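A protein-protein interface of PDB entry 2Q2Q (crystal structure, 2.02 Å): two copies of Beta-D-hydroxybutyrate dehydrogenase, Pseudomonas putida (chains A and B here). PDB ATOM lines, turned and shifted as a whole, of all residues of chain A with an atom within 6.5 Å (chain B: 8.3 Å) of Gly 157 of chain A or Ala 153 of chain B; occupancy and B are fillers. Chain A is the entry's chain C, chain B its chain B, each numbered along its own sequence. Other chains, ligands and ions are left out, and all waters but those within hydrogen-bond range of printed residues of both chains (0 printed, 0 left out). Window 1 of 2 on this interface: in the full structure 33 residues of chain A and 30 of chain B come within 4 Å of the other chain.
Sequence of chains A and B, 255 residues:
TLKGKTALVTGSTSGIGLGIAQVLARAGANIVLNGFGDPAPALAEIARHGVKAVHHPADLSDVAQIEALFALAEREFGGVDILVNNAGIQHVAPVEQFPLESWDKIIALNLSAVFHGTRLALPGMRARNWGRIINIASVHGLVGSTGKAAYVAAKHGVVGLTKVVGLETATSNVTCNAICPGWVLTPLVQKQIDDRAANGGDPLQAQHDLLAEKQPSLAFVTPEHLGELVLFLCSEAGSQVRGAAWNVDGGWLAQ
The backbone carbonyl oxygen of His 140 of chain B sits at hydrogen-bond distance from a ring nitrogen (ND1) of His 156 of chain B (2.9 Å).
A ring nitrogen (ND1) of His 156 of chain B sits close to the backbone carbonyl oxygen of Gly 141 of chain B (3.4 Å).
O of Val 152 of chain B is in hydrogen-bond range of ND1 of His 156 of chain B, 3.0 Å away.
O of Gly 141 of chain A lies close to ND1 of His 156 of chain A (3.5 Å).
Gly 157 of chain A touches just these residues of chain B: Ala 153 (3.3 Å) and Gly 157 (3.8 Å).
Printed residues of chain A within 4 Å of Ala 153 of chain B: Leu 111 and Gly 157.
Of the printed residues of chain A, Val 152 of chain B touches Gly 160 and Val 164.
Of the printed residues of chain B, Ala 153 of chain A touches Gly 157.
Leu 161 of chain B touches none of the printed residues of chain A.
Gly 141 of chain B touches none of the printed residues of chain A.
The nearest printed residue of chain A that does not touch Ala 153 of chain B is Leu 161 of chain A (4.4 Å).
The nearest printed residue of chain A that does not touch Val 152 of chain B is Leu 161 of chain A (4.4 Å).
Hydrophobic or aromatic side chains of chain B within 4 Å of the printed part of chain A: Ala 149, Val 152, Ala 153 and His 156.
Hydrophobic or aromatic side chains of chain A that line the printed part of chain B: Leu 111, Val 152, Ala 153, His 156, Leu 161 and Val 164.
Along chain A the printed residues that touch a printed residue of chain B span positions 111 to 164.
Val 152 of chain A touches Gly 160 of chain B, and with the chains exchanged Gly 160 of chain A touches Val 152 of chain B.
His 156 of chain A touches Gly 157 of chain B, but with the chains exchanged Gly 157 of chain A does not touch His 156 of chain B (4.05 Å).
His 156 of chain A touches Gly 160 of chain B, and with the chains exchanged Gly 160 of chain A touches His 156 of chain B.
Gly 157 of chain B touches its own counterpart, Gly 157 of chain A.
12 positions are printed for both chains.
Of the 13 pairs that touch across the chains among the printed residues, 8 have their exchanged pair printed and touching as well.
CB of Ala 153 of chain B touches CD1 of Leu 111 of chain A, at 3.98 Å.
Ala 153 of chain A touches Gly 157 of chain B (O to CA, 3.2 Å).
His 156 of chain A touches His 156 of chain B.
His 156 of chain A touches Gly 157 of chain B.
His 156 of chain A touches Gly 160 of chain B.
CA of Gly 157 of chain A touches O of Ala 153 of chain B, at 3.3 Å.
N of Gly 157 of chain A touches N of Gly 157 of chain B, at 3.8 Å.
Gly 160 of chain A touches His 156 of chain B (CA to NE2, 3.5 Å).
Leu 161 of chain A touches Ala 149 of chain B.
Val 164 of chain A touches Ala 149 of chain B.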
ATOM      1  N   LEU A 111     -19.640  14.681  22.556  1.00  0.00           N
ATOM      2  CA  LEU A 111     -18.267  15.197  22.199  1.00  0.00           C
ATOM      3  C   LEU A 111     -17.165  14.393  22.902  1.00  0.00           C
ATOM      4  O   LEU A 111     -16.291  13.863  22.246  1.00  0.00           O
ATOM      5  CB  LEU A 111     -18.162  16.716  22.493  1.00  0.00           C
ATOM      6  CG  LEU A 111     -16.747  17.372  22.439  1.00  0.00           C
ATOM      7  CD1 LEU A 111     -16.057  17.292  21.054  1.00  0.00           C
ATOM      8  CD2 LEU A 111     -16.891  18.801  22.843  1.00  0.00           C
ATOM      9  N   GLY A 141     -22.860  20.878  13.270  1.00  0.00           N
ATOM     10  CA  GLY A 141     -21.472  21.044  13.563  1.00  0.00           C
ATOM     11  C   GLY A 141     -20.890  22.078  12.637  1.00  0.00           C
ATOM     12  O   GLY A 141     -19.710  22.439  12.771  1.00  0.00           O
ATOM     13  N   VAL A 152     -25.363  21.824  19.250  1.00  0.00           N
ATOM     14  CA  VAL A 152     -24.539  22.592  18.336  1.00  0.00           C
ATOM     15  C   VAL A 152     -23.088  22.688  18.898  1.00  0.00           C
ATOM     16  O   VAL A 152     -22.174  22.363  18.203  1.00  0.00           O
ATOM     17  CB  VAL A 152     -25.207  23.934  17.826  1.00  0.00           C
ATOM     18  CG1 VAL A 152     -24.254  24.698  16.888  1.00  0.00           C
ATOM     19  CG2 VAL A 152     -26.553  23.645  17.066  1.00  0.00           C
ATOM     20  N   ALA A 153     -22.897  22.997  20.183  1.00  0.00           N
ATOM     21  CA  ALA A 153     -21.552  23.112  20.716  1.00  0.00           C
ATOM     22  C   ALA A 153     -20.824  21.779  20.548  1.00  0.00           C
ATOM     23  O   ALA A 153     -19.703  21.770  20.041  1.00  0.00           O
ATOM     24  CB  ALA A 153     -21.565  23.536  22.203  1.00  0.00           C
ATOM     25  N   ALA A 154     -21.453  20.662  20.969  1.00  0.00           N
ATOM     26  CA  ALA A 154     -20.834  19.332  20.856  1.00  0.00           C
ATOM     27  C   ALA A 154     -20.453  18.955  19.416  1.00  0.00           C
ATOM     28  O   ALA A 154     -19.336  18.559  19.125  1.00  0.00           O
ATOM     29  CB  ALA A 154     -21.776  18.204  21.579  1.00  0.00           C
ATOM     30  N   LYS A 155     -21.358  19.139  18.464  1.00  0.00           N
ATOM     31  CA  LYS A 155     -21.051  18.776  17.087  1.00  0.00           C
ATOM     32  C   LYS A 155     -20.027  19.734  16.387  1.00  0.00           C
ATOM     33  O   LYS A 155     -19.247  19.269  15.609  1.00  0.00           O
ATOM     34  CB  LYS A 155     -22.325  18.637  16.234  1.00  0.00           C
ATOM     35  CG  LYS A 155     -23.262  17.511  16.724  1.00  0.00           C
ATOM     36  CD  LYS A 155     -22.652  16.100  16.485  1.00  0.00           C
ATOM     37  CE  LYS A 155     -23.567  15.040  17.003  1.00  0.00           C
ATOM     38  NZ  LYS A 155     -23.459  13.689  16.357  1.00  0.00           N
ATOM     39  N   HIS A 156     -20.032  21.031  16.688  1.00  0.00           N
ATOM     40  CA  HIS A 156     -18.934  21.892  16.274  1.00  0.00           C
ATOM     41  C   HIS A 156     -17.633  21.345  16.872  1.00  0.00           C
ATOM     42  O   HIS A 156     -16.587  21.306  16.189  1.00  0.00           O
ATOM     43  CB  HIS A 156     -19.184  23.377  16.635  1.00  0.00           C
ATOM     44  CG  HIS A 156     -20.127  24.094  15.696  1.00  0.00           C
ATOM     45  ND1 HIS A 156     -19.740  25.163  14.909  1.00  0.00           N
ATOM     46  CD2 HIS A 156     -21.448  23.894  15.439  1.00  0.00           C
ATOM     47  CE1 HIS A 156     -20.758  25.539  14.144  1.00  0.00           C
ATOM     48  NE2 HIS A 156     -21.819  24.807  14.471  1.00  0.00           N
ATOM     49  N   GLY A 157     -17.652  20.936  18.132  1.00  0.00           N
ATOM     50  CA  GLY A 157     -16.418  20.404  18.737  1.00  0.00           C
ATOM     51  C   GLY A 157     -15.918  19.195  17.996  1.00  0.00           C
ATOM     52  O   GLY A 157     -14.713  19.018  17.784  1.00  0.00           O
ATOM     53  N   VAL A 158     -16.833  18.318  17.618  1.00  0.00           N
ATOM     54  CA  VAL A 158     -16.449  17.101  16.865  1.00  0.00           C
ATOM     55  C   VAL A 158     -15.773  17.415  15.512  1.00  0.00           C
ATOM     56  O   VAL A 158     -14.693  16.826  15.125  1.00  0.00           O
ATOM     57  CB  VAL A 158     -17.705  16.166  16.705  1.00  0.00           C
ATOM     58  CG1 VAL A 158     -17.461  15.062  15.660  1.00  0.00           C
ATOM     59  CG2 VAL A 158     -18.004  15.529  18.013  1.00  0.00           C
ATOM     60  N   VAL A 159     -16.379  18.362  14.789  1.00  0.00           N
ATOM     61  CA  VAL A 159     -15.804  18.881  13.568  1.00  0.00           C
ATOM     62  C   VAL A 159     -14.380  19.423  13.833  1.00  0.00           C
ATOM     63  O   VAL A 159     -13.489  19.080  13.143  1.00  0.00           O
ATOM     64  CB  VAL A 159     -16.728  19.873  12.834  1.00  0.00           C
ATOM     65  CG1 VAL A 159     -15.949  20.665  11.732  1.00  0.00           C
ATOM     66  CG2 VAL A 159     -17.926  19.150  12.180  1.00  0.00           C
ATOM     67  N   GLY A 160     -14.161  20.194  14.869  1.00  0.00           N
ATOM     68  CA  GLY A 160     -12.803  20.694  15.165  1.00  0.00           C
ATOM     69  C   GLY A 160     -11.909  19.550  15.577  1.00  0.00           C
ATOM     70  O   GLY A 160     -10.815  19.436  15.108  1.00  0.00           O
ATOM     71  N   LEU A 161     -12.371  18.672  16.455  1.00  0.00           N
ATOM     72  CA  LEU A 161     -11.494  17.544  16.846  1.00  0.00           C
ATOM     73  C   LEU A 161     -11.014  16.718  15.620  1.00  0.00           C
ATOM     74  O   LEU A 161      -9.838  16.200  15.534  1.00  0.00           O
ATOM     75  CB  LEU A 161     -12.263  16.672  17.866  1.00  0.00           C
ATOM     76  CG  LEU A 161     -11.607  15.338  18.256  1.00  0.00           C
ATOM     77  CD1 LEU A 161     -10.399  15.632  19.122  1.00  0.00           C
ATOM     78  CD2 LEU A 161     -12.660  14.535  19.030  1.00  0.00           C
ATOM     79  N   THR A 162     -11.928  16.541  14.697  1.00  0.00           N
ATOM     80  CA  THR A 162     -11.697  15.775  13.492  1.00  0.00           C
ATOM     81  C   THR A 162     -10.539  16.356  12.659  1.00  0.00           C
ATOM     82  O   THR A 162      -9.647  15.617  12.133  1.00  0.00           O
ATOM     83  CB  THR A 162     -12.942  15.737  12.602  1.00  0.00           C
ATOM     84  OG1 THR A 162     -14.020  15.057  13.238  1.00  0.00           O
ATOM     85  CG2 THR A 162     -12.654  15.021  11.328  1.00  0.00           C
ATOM     86  N   VAL A 164      -8.042  18.166  13.977  1.00  0.00           N
ATOM     87  CA  VAL A 164      -6.784  17.871  14.712  1.00  0.00           C
ATOM     88  C   VAL A 164      -6.253  16.469  14.421  1.00  0.00           C
ATOM     89  O   VAL A 164      -5.093  16.303  14.070  1.00  0.00           O
ATOM     90  CB  VAL A 164      -6.978  18.020  16.206  1.00  0.00           C
ATOM     91  CG1 VAL A 164      -5.671  17.593  16.967  1.00  0.00           C
ATOM     92  CG2 VAL A 164      -7.390  19.486  16.506  1.00  0.00           C
ATOM     93  N   TRP B 103      -8.083  17.351  28.846  1.00  0.00           N
ATOM     94  CA  TRP B 103      -9.286  17.366  28.026  1.00  0.00           C
ATOM     95  C   TRP B 103     -10.443  17.941  28.864  1.00  0.00           C
ATOM     96  O   TRP B 103     -11.084  18.830  28.472  1.00  0.00           O
ATOM     97  CB  TRP B 103      -9.641  15.938  27.535  1.00  0.00           C
ATOM     98  CG  TRP B 103     -10.967  15.921  26.818  1.00  0.00           C
ATOM     99  CD1 TRP B 103     -12.241  15.712  27.398  1.00  0.00           C
ATOM    100  CD2 TRP B 103     -11.195  16.134  25.411  1.00  0.00           C
ATOM    101  NE1 TRP B 103     -13.203  15.801  26.403  1.00  0.00           N
ATOM    102  CE2 TRP B 103     -12.597  16.085  25.199  1.00  0.00           C
ATOM    103  CE3 TRP B 103     -10.356  16.413  24.311  1.00  0.00           C
ATOM    104  CZ2 TRP B 103     -13.166  16.287  23.938  1.00  0.00           C
ATOM    105  CZ3 TRP B 103     -10.927  16.639  23.077  1.00  0.00           C
ATOM    106  CH2 TRP B 103     -12.333  16.560  22.895  1.00  0.00           C
ATOM    107  N   ILE B 106     -10.106  21.714  29.834  1.00  0.00           N
ATOM    108  CA  ILE B 106     -10.131  22.568  28.671  1.00  0.00           C
ATOM    109  C   ILE B 106     -11.582  22.671  28.218  1.00  0.00           C
ATOM    110  O   ILE B 106     -12.055  23.742  28.008  1.00  0.00           O
ATOM    111  CB  ILE B 106      -9.168  22.112  27.601  1.00  0.00           C
ATOM    112  CG1 ILE B 106      -7.793  22.552  28.010  1.00  0.00           C
ATOM    113  CG2 ILE B 106      -9.470  22.816  26.304  1.00  0.00           C
ATOM    114  CD1 ILE B 106      -6.765  21.960  27.265  1.00  0.00           C
ATOM    115  N   ILE B 107     -12.293  21.563  28.094  1.00  0.00           N
ATOM    116  CA  ILE B 107     -13.710  21.635  27.840  1.00  0.00           C
ATOM    117  C   ILE B 107     -14.509  22.487  28.892  1.00  0.00           C
ATOM    118  O   ILE B 107     -15.341  23.310  28.505  1.00  0.00           O
ATOM    119  CB  ILE B 107     -14.224  20.210  27.783  1.00  0.00           C
ATOM    120  CG1 ILE B 107     -13.496  19.505  26.638  1.00  0.00           C
ATOM    121  CG2 ILE B 107     -15.773  20.155  27.679  1.00  0.00           C
ATOM    122  CD1 ILE B 107     -13.741  20.222  25.254  1.00  0.00           C
ATOM    123  N   ASN B 110     -12.925  26.415  28.632  1.00  0.00           N
ATOM    124  CA  ASN B 110     -13.093  27.045  27.305  1.00  0.00           C
ATOM    125  C   ASN B 110     -14.445  26.914  26.688  1.00  0.00           C
ATOM    126  O   ASN B 110     -14.787  27.711  25.797  1.00  0.00           O
ATOM    127  CB  ASN B 110     -12.085  26.541  26.282  1.00  0.00           C
ATOM    128  CG  ASN B 110     -10.698  27.100  26.515  1.00  0.00           C
ATOM    129  OD1 ASN B 110     -10.550  28.276  26.746  1.00  0.00           O
ATOM    130  ND2 ASN B 110      -9.697  26.284  26.431  1.00  0.00           N
ATOM    131  N   LEU B 111     -15.196  25.888  27.070  1.00  0.00           N
ATOM    132  CA  LEU B 111     -16.482  25.751  26.437  1.00  0.00           C
ATOM    133  C   LEU B 111     -17.607  25.892  27.450  1.00  0.00           C
ATOM    134  O   LEU B 111     -18.381  26.798  27.351  1.00  0.00           O
ATOM    135  CB  LEU B 111     -16.560  24.470  25.605  1.00  0.00           C
ATOM    136  CG  LEU B 111     -17.934  24.095  25.039  1.00  0.00           C
ATOM    137  CD1 LEU B 111     -18.489  25.239  24.178  1.00  0.00           C
ATOM    138  CD2 LEU B 111     -17.847  22.760  24.282  1.00  0.00           C
ATOM    139  N   HIS B 140      -8.785  28.665  16.256  1.00  0.00           N
ATOM    140  CA  HIS B 140      -8.971  27.229  16.520  1.00  0.00           C
ATOM    141  C   HIS B 140     -10.444  26.913  16.861  1.00  0.00           C
ATOM    142  O   HIS B 140     -10.782  25.807  17.167  1.00  0.00           O
ATOM    143  CB  HIS B 140      -7.986  26.832  17.589  1.00  0.00           C
ATOM    144  CG  HIS B 140      -6.572  26.787  17.079  1.00  0.00           C
ATOM    145  ND1 HIS B 140      -6.202  26.073  15.950  1.00  0.00           N
ATOM    146  CD2 HIS B 140      -5.431  27.283  17.595  1.00  0.00           C
ATOM    147  CE1 HIS B 140      -4.891  26.130  15.798  1.00  0.00           C
ATOM    148  NE2 HIS B 140      -4.399  26.878  16.769  1.00  0.00           N
ATOM    149  N   GLY B 141     -11.309  27.916  16.755  1.00  0.00           N
ATOM    150  CA  GLY B 141     -12.761  27.738  16.671  1.00  0.00           C
ATOM    151  C   GLY B 141     -13.127  27.509  15.212  1.00  0.00           C
ATOM    152  O   GLY B 141     -14.262  27.087  14.913  1.00  0.00           O
ATOM    153  N   VAL B 143     -10.358  26.364  12.485  1.00  0.00           N
ATOM    154  CA  VAL B 143      -9.517  25.315  11.921  1.00  0.00           C
ATOM    155  C   VAL B 143      -8.891  24.520  13.063  1.00  0.00           C
ATOM    156  O   VAL B 143      -9.002  24.939  14.231  1.00  0.00           O
ATOM    157  CB  VAL B 143      -8.366  25.905  10.970  1.00  0.00           C
ATOM    158  CG1 VAL B 143      -8.966  26.533   9.711  1.00  0.00           C
ATOM    159  CG2 VAL B 143      -7.468  26.928  11.721  1.00  0.00           C
ATOM    160  N   GLY B 144      -8.177  23.431  12.708  1.00  0.00           N
ATOM    161  CA  GLY B 144      -7.385  22.633  13.648  1.00  0.00           C
ATOM    162  C   GLY B 144      -5.883  22.994  13.588  1.00  0.00           C
ATOM    163  O   GLY B 144      -5.455  23.730  12.663  1.00  0.00           O
ATOM    164  N   LYS B 148      -3.476  19.865  19.437  1.00  0.00           N
ATOM    165  CA  LYS B 148      -4.426  20.691  20.221  1.00  0.00           C
ATOM    166  C   LYS B 148      -5.877  20.213  20.263  1.00  0.00           C
ATOM    167  O   LYS B 148      -6.777  21.010  20.164  1.00  0.00           O
ATOM    168  CB  LYS B 148      -4.363  22.164  19.831  1.00  0.00           C
ATOM    169  CG  LYS B 148      -2.949  22.729  19.888  1.00  0.00           C
ATOM    170  CD  LYS B 148      -2.861  24.216  19.352  1.00  0.00           C
ATOM    171  CE  LYS B 148      -1.475  24.787  19.554  1.00  0.00           C
ATOM    172  NZ  LYS B 148      -1.371  26.252  19.387  1.00  0.00           N
ATOM    173  N   ALA B 149      -6.070  18.935  20.552  1.00  0.00           N
ATOM    174  CA  ALA B 149      -7.362  18.231  20.461  1.00  0.00           C
ATOM    175  C   ALA B 149      -8.439  18.885  21.267  1.00  0.00           C
ATOM    176  O   ALA B 149      -9.495  19.217  20.742  1.00  0.00           O
ATOM    177  CB  ALA B 149      -7.188  16.810  20.906  1.00  0.00           C
ATOM    178  N   ALA B 150      -8.145  19.138  22.538  1.00  0.00           N
ATOM    179  CA  ALA B 150      -9.129  19.741  23.480  1.00  0.00           C
ATOM    180  C   ALA B 150      -9.425  21.186  23.179  1.00  0.00           C
ATOM    181  O   ALA B 150     -10.574  21.645  23.208  1.00  0.00           O
ATOM    182  CB  ALA B 150      -8.661  19.534  24.937  1.00  0.00           C
ATOM    183  N   TYR B 151      -8.388  21.938  22.864  1.00  0.00           N
ATOM    184  CA  TYR B 151      -8.546  23.346  22.629  1.00  0.00           C
ATOM    185  C   TYR B 151      -9.453  23.614  21.389  1.00  0.00           C
ATOM    186  O   TYR B 151     -10.413  24.434  21.393  1.00  0.00           O
ATOM    187  CB  TYR B 151      -7.178  24.031  22.540  1.00  0.00           C
ATOM    188  CG  TYR B 151      -7.179  25.590  22.470  1.00  0.00           C
ATOM    189  CD1 TYR B 151      -7.159  26.266  21.252  1.00  0.00           C
ATOM    190  CD2 TYR B 151      -7.114  26.358  23.628  1.00  0.00           C
ATOM    191  CE1 TYR B 151      -7.146  27.706  21.229  1.00  0.00           C
ATOM    192  CE2 TYR B 151      -7.078  27.742  23.614  1.00  0.00           C
ATOM    193  CZ  TYR B 151      -7.090  28.410  22.445  1.00  0.00           C
ATOM    194  OH  TYR B 151      -7.040  29.780  22.521  1.00  0.00           O
ATOM    195  N   VAL B 152      -9.133  22.900  20.347  1.00  0.00           N
ATOM    196  CA  VAL B 152      -9.824  23.042  19.064  1.00  0.00           C
ATOM    197  C   VAL B 152     -11.299  22.646  19.155  1.00  0.00           C
ATOM    198  O   VAL B 152     -12.161  23.376  18.690  1.00  0.00           O
ATOM    199  CB  VAL B 152      -9.058  22.303  17.897  1.00  0.00           C
ATOM    200  CG1 VAL B 152      -9.934  22.351  16.613  1.00  0.00           C
ATOM    201  CG2 VAL B 152      -7.601  22.964  17.629  1.00  0.00           C
ATOM    202  N   ALA B 153     -11.585  21.489  19.790  1.00  0.00           N
ATOM    203  CA  ALA B 153     -12.937  21.097  20.182  1.00  0.00           C
ATOM    204  C   ALA B 153     -13.690  22.124  21.005  1.00  0.00           C
ATOM    205  O   ALA B 153     -14.790  22.522  20.614  1.00  0.00           O
ATOM    206  CB  ALA B 153     -12.890  19.705  20.942  1.00  0.00           C
ATOM    207  N   ALA B 154     -13.125  22.567  22.143  1.00  0.00           N
ATOM    208  CA  ALA B 154     -13.726  23.623  22.944  1.00  0.00           C
ATOM    209  C   ALA B 154     -14.063  24.927  22.109  1.00  0.00           C
ATOM    210  O   ALA B 154     -15.200  25.379  22.054  1.00  0.00           O
ATOM    211  CB  ALA B 154     -12.819  23.935  24.170  1.00  0.00           C
ATOM    212  N   LYS B 155     -13.081  25.470  21.416  1.00  0.00           N
ATOM    213  CA  LYS B 155     -13.231  26.750  20.650  1.00  0.00           C
ATOM    214  C   LYS B 155     -14.209  26.559  19.489  1.00  0.00           C
ATOM    215  O   LYS B 155     -15.058  27.435  19.246  1.00  0.00           O
ATOM    216  CB  LYS B 155     -11.873  27.262  20.191  1.00  0.00           C
ATOM    217  CG  LYS B 155     -10.869  27.759  21.259  1.00  0.00           C
ATOM    218  CD  LYS B 155     -11.425  28.893  22.203  1.00  0.00           C
ATOM    219  CE  LYS B 155     -10.326  29.512  23.131  1.00  0.00           C
ATOM    220  NZ  LYS B 155     -10.974  30.671  23.900  1.00  0.00           N
ATOM    221  N   HIS B 156     -14.142  25.419  18.794  1.00  0.00           N
ATOM    222  CA  HIS B 156     -15.177  25.126  17.798  1.00  0.00           C
ATOM    223  C   HIS B 156     -16.623  25.081  18.437  1.00  0.00           C
ATOM    224  O   HIS B 156     -17.605  25.595  17.853  1.00  0.00           O
ATOM    225  CB  HIS B 156     -14.900  23.787  17.114  1.00  0.00           C
ATOM    226  CG  HIS B 156     -14.107  23.878  15.837  1.00  0.00           C
ATOM    227  ND1 HIS B 156     -12.766  24.123  15.834  1.00  0.00           N
ATOM    228  CD2 HIS B 156     -14.453  23.695  14.542  1.00  0.00           C
ATOM    229  CE1 HIS B 156     -12.316  24.154  14.587  1.00  0.00           C
ATOM    230  NE2 HIS B 156     -13.312  23.846  13.790  1.00  0.00           N
ATOM    231  N   GLY B 157     -16.757  24.384  19.560  1.00  0.00           N
ATOM    232  CA  GLY B 157     -17.980  24.437  20.370  1.00  0.00           C
ATOM    233  C   GLY B 157     -18.428  25.861  20.698  1.00  0.00           C
ATOM    234  O   GLY B 157     -19.638  26.171  20.615  1.00  0.00           O
ATOM    235  N   VAL B 158     -17.528  26.734  21.130  1.00  0.00           N
ATOM    236  CA  VAL B 158     -17.910  28.142  21.390  1.00  0.00           C
ATOM    237  C   VAL B 158     -18.484  28.801  20.133  1.00  0.00           C
ATOM    238  O   VAL B 158     -19.463  29.635  20.192  1.00  0.00           O
ATOM    239  CB  VAL B 158     -16.708  29.021  21.831  1.00  0.00           C
ATOM    240  CG1 VAL B 158     -17.157  30.459  22.038  1.00  0.00           C
ATOM    241  CG2 VAL B 158     -16.106  28.535  23.163  1.00  0.00           C
ATOM    242  N   VAL B 159     -17.803  28.589  19.007  1.00  0.00           N
ATOM    243  CA  VAL B 159     -18.252  29.228  17.755  1.00  0.00           C
ATOM    244  C   VAL B 159     -19.666  28.713  17.441  1.00  0.00           C
ATOM    245  O   VAL B 159     -20.529  29.488  17.028  1.00  0.00           O
ATOM    246  CB  VAL B 159     -17.321  28.910  16.676  1.00  0.00           C
ATOM    247  CG1 VAL B 159     -17.975  29.089  15.326  1.00  0.00           C
ATOM    248  CG2 VAL B 159     -15.973  29.841  16.749  1.00  0.00           C
ATOM    249  N   GLY B 160     -19.931  27.409  17.667  1.00  0.00           N
ATOM    250  CA  GLY B 160     -21.297  26.870  17.479  1.00  0.00           C
ATOM    251  C   GLY B 160     -22.334  27.371  18.451  1.00  0.00           C
ATOM    252  O   GLY B 160     -23.443  27.719  18.042  1.00  0.00           O
ATOM    253  N   LEU B 161     -22.031  27.332  19.762  1.00  0.00           N
ATOM    254  CA  LEU B 161     -22.826  27.942  20.779  1.00  0.00           C
ATOM    255  C   LEU B 161     -23.100  29.421  20.521  1.00  0.00           C
ATOM    256  O   LEU B 161     -24.230  29.853  20.781  1.00  0.00           O
ATOM    257  CB  LEU B 161     -22.156  27.823  22.162  1.00  0.00           C
ATOM    258  CG  LEU B 161     -22.910  28.436  23.355  1.00  0.00           C
ATOM    259  CD1 LEU B 161     -24.320  27.807  23.611  1.00  0.00           C
ATOM    260  CD2 LEU B 161     -22.004  28.294  24.621  1.00  0.00           C
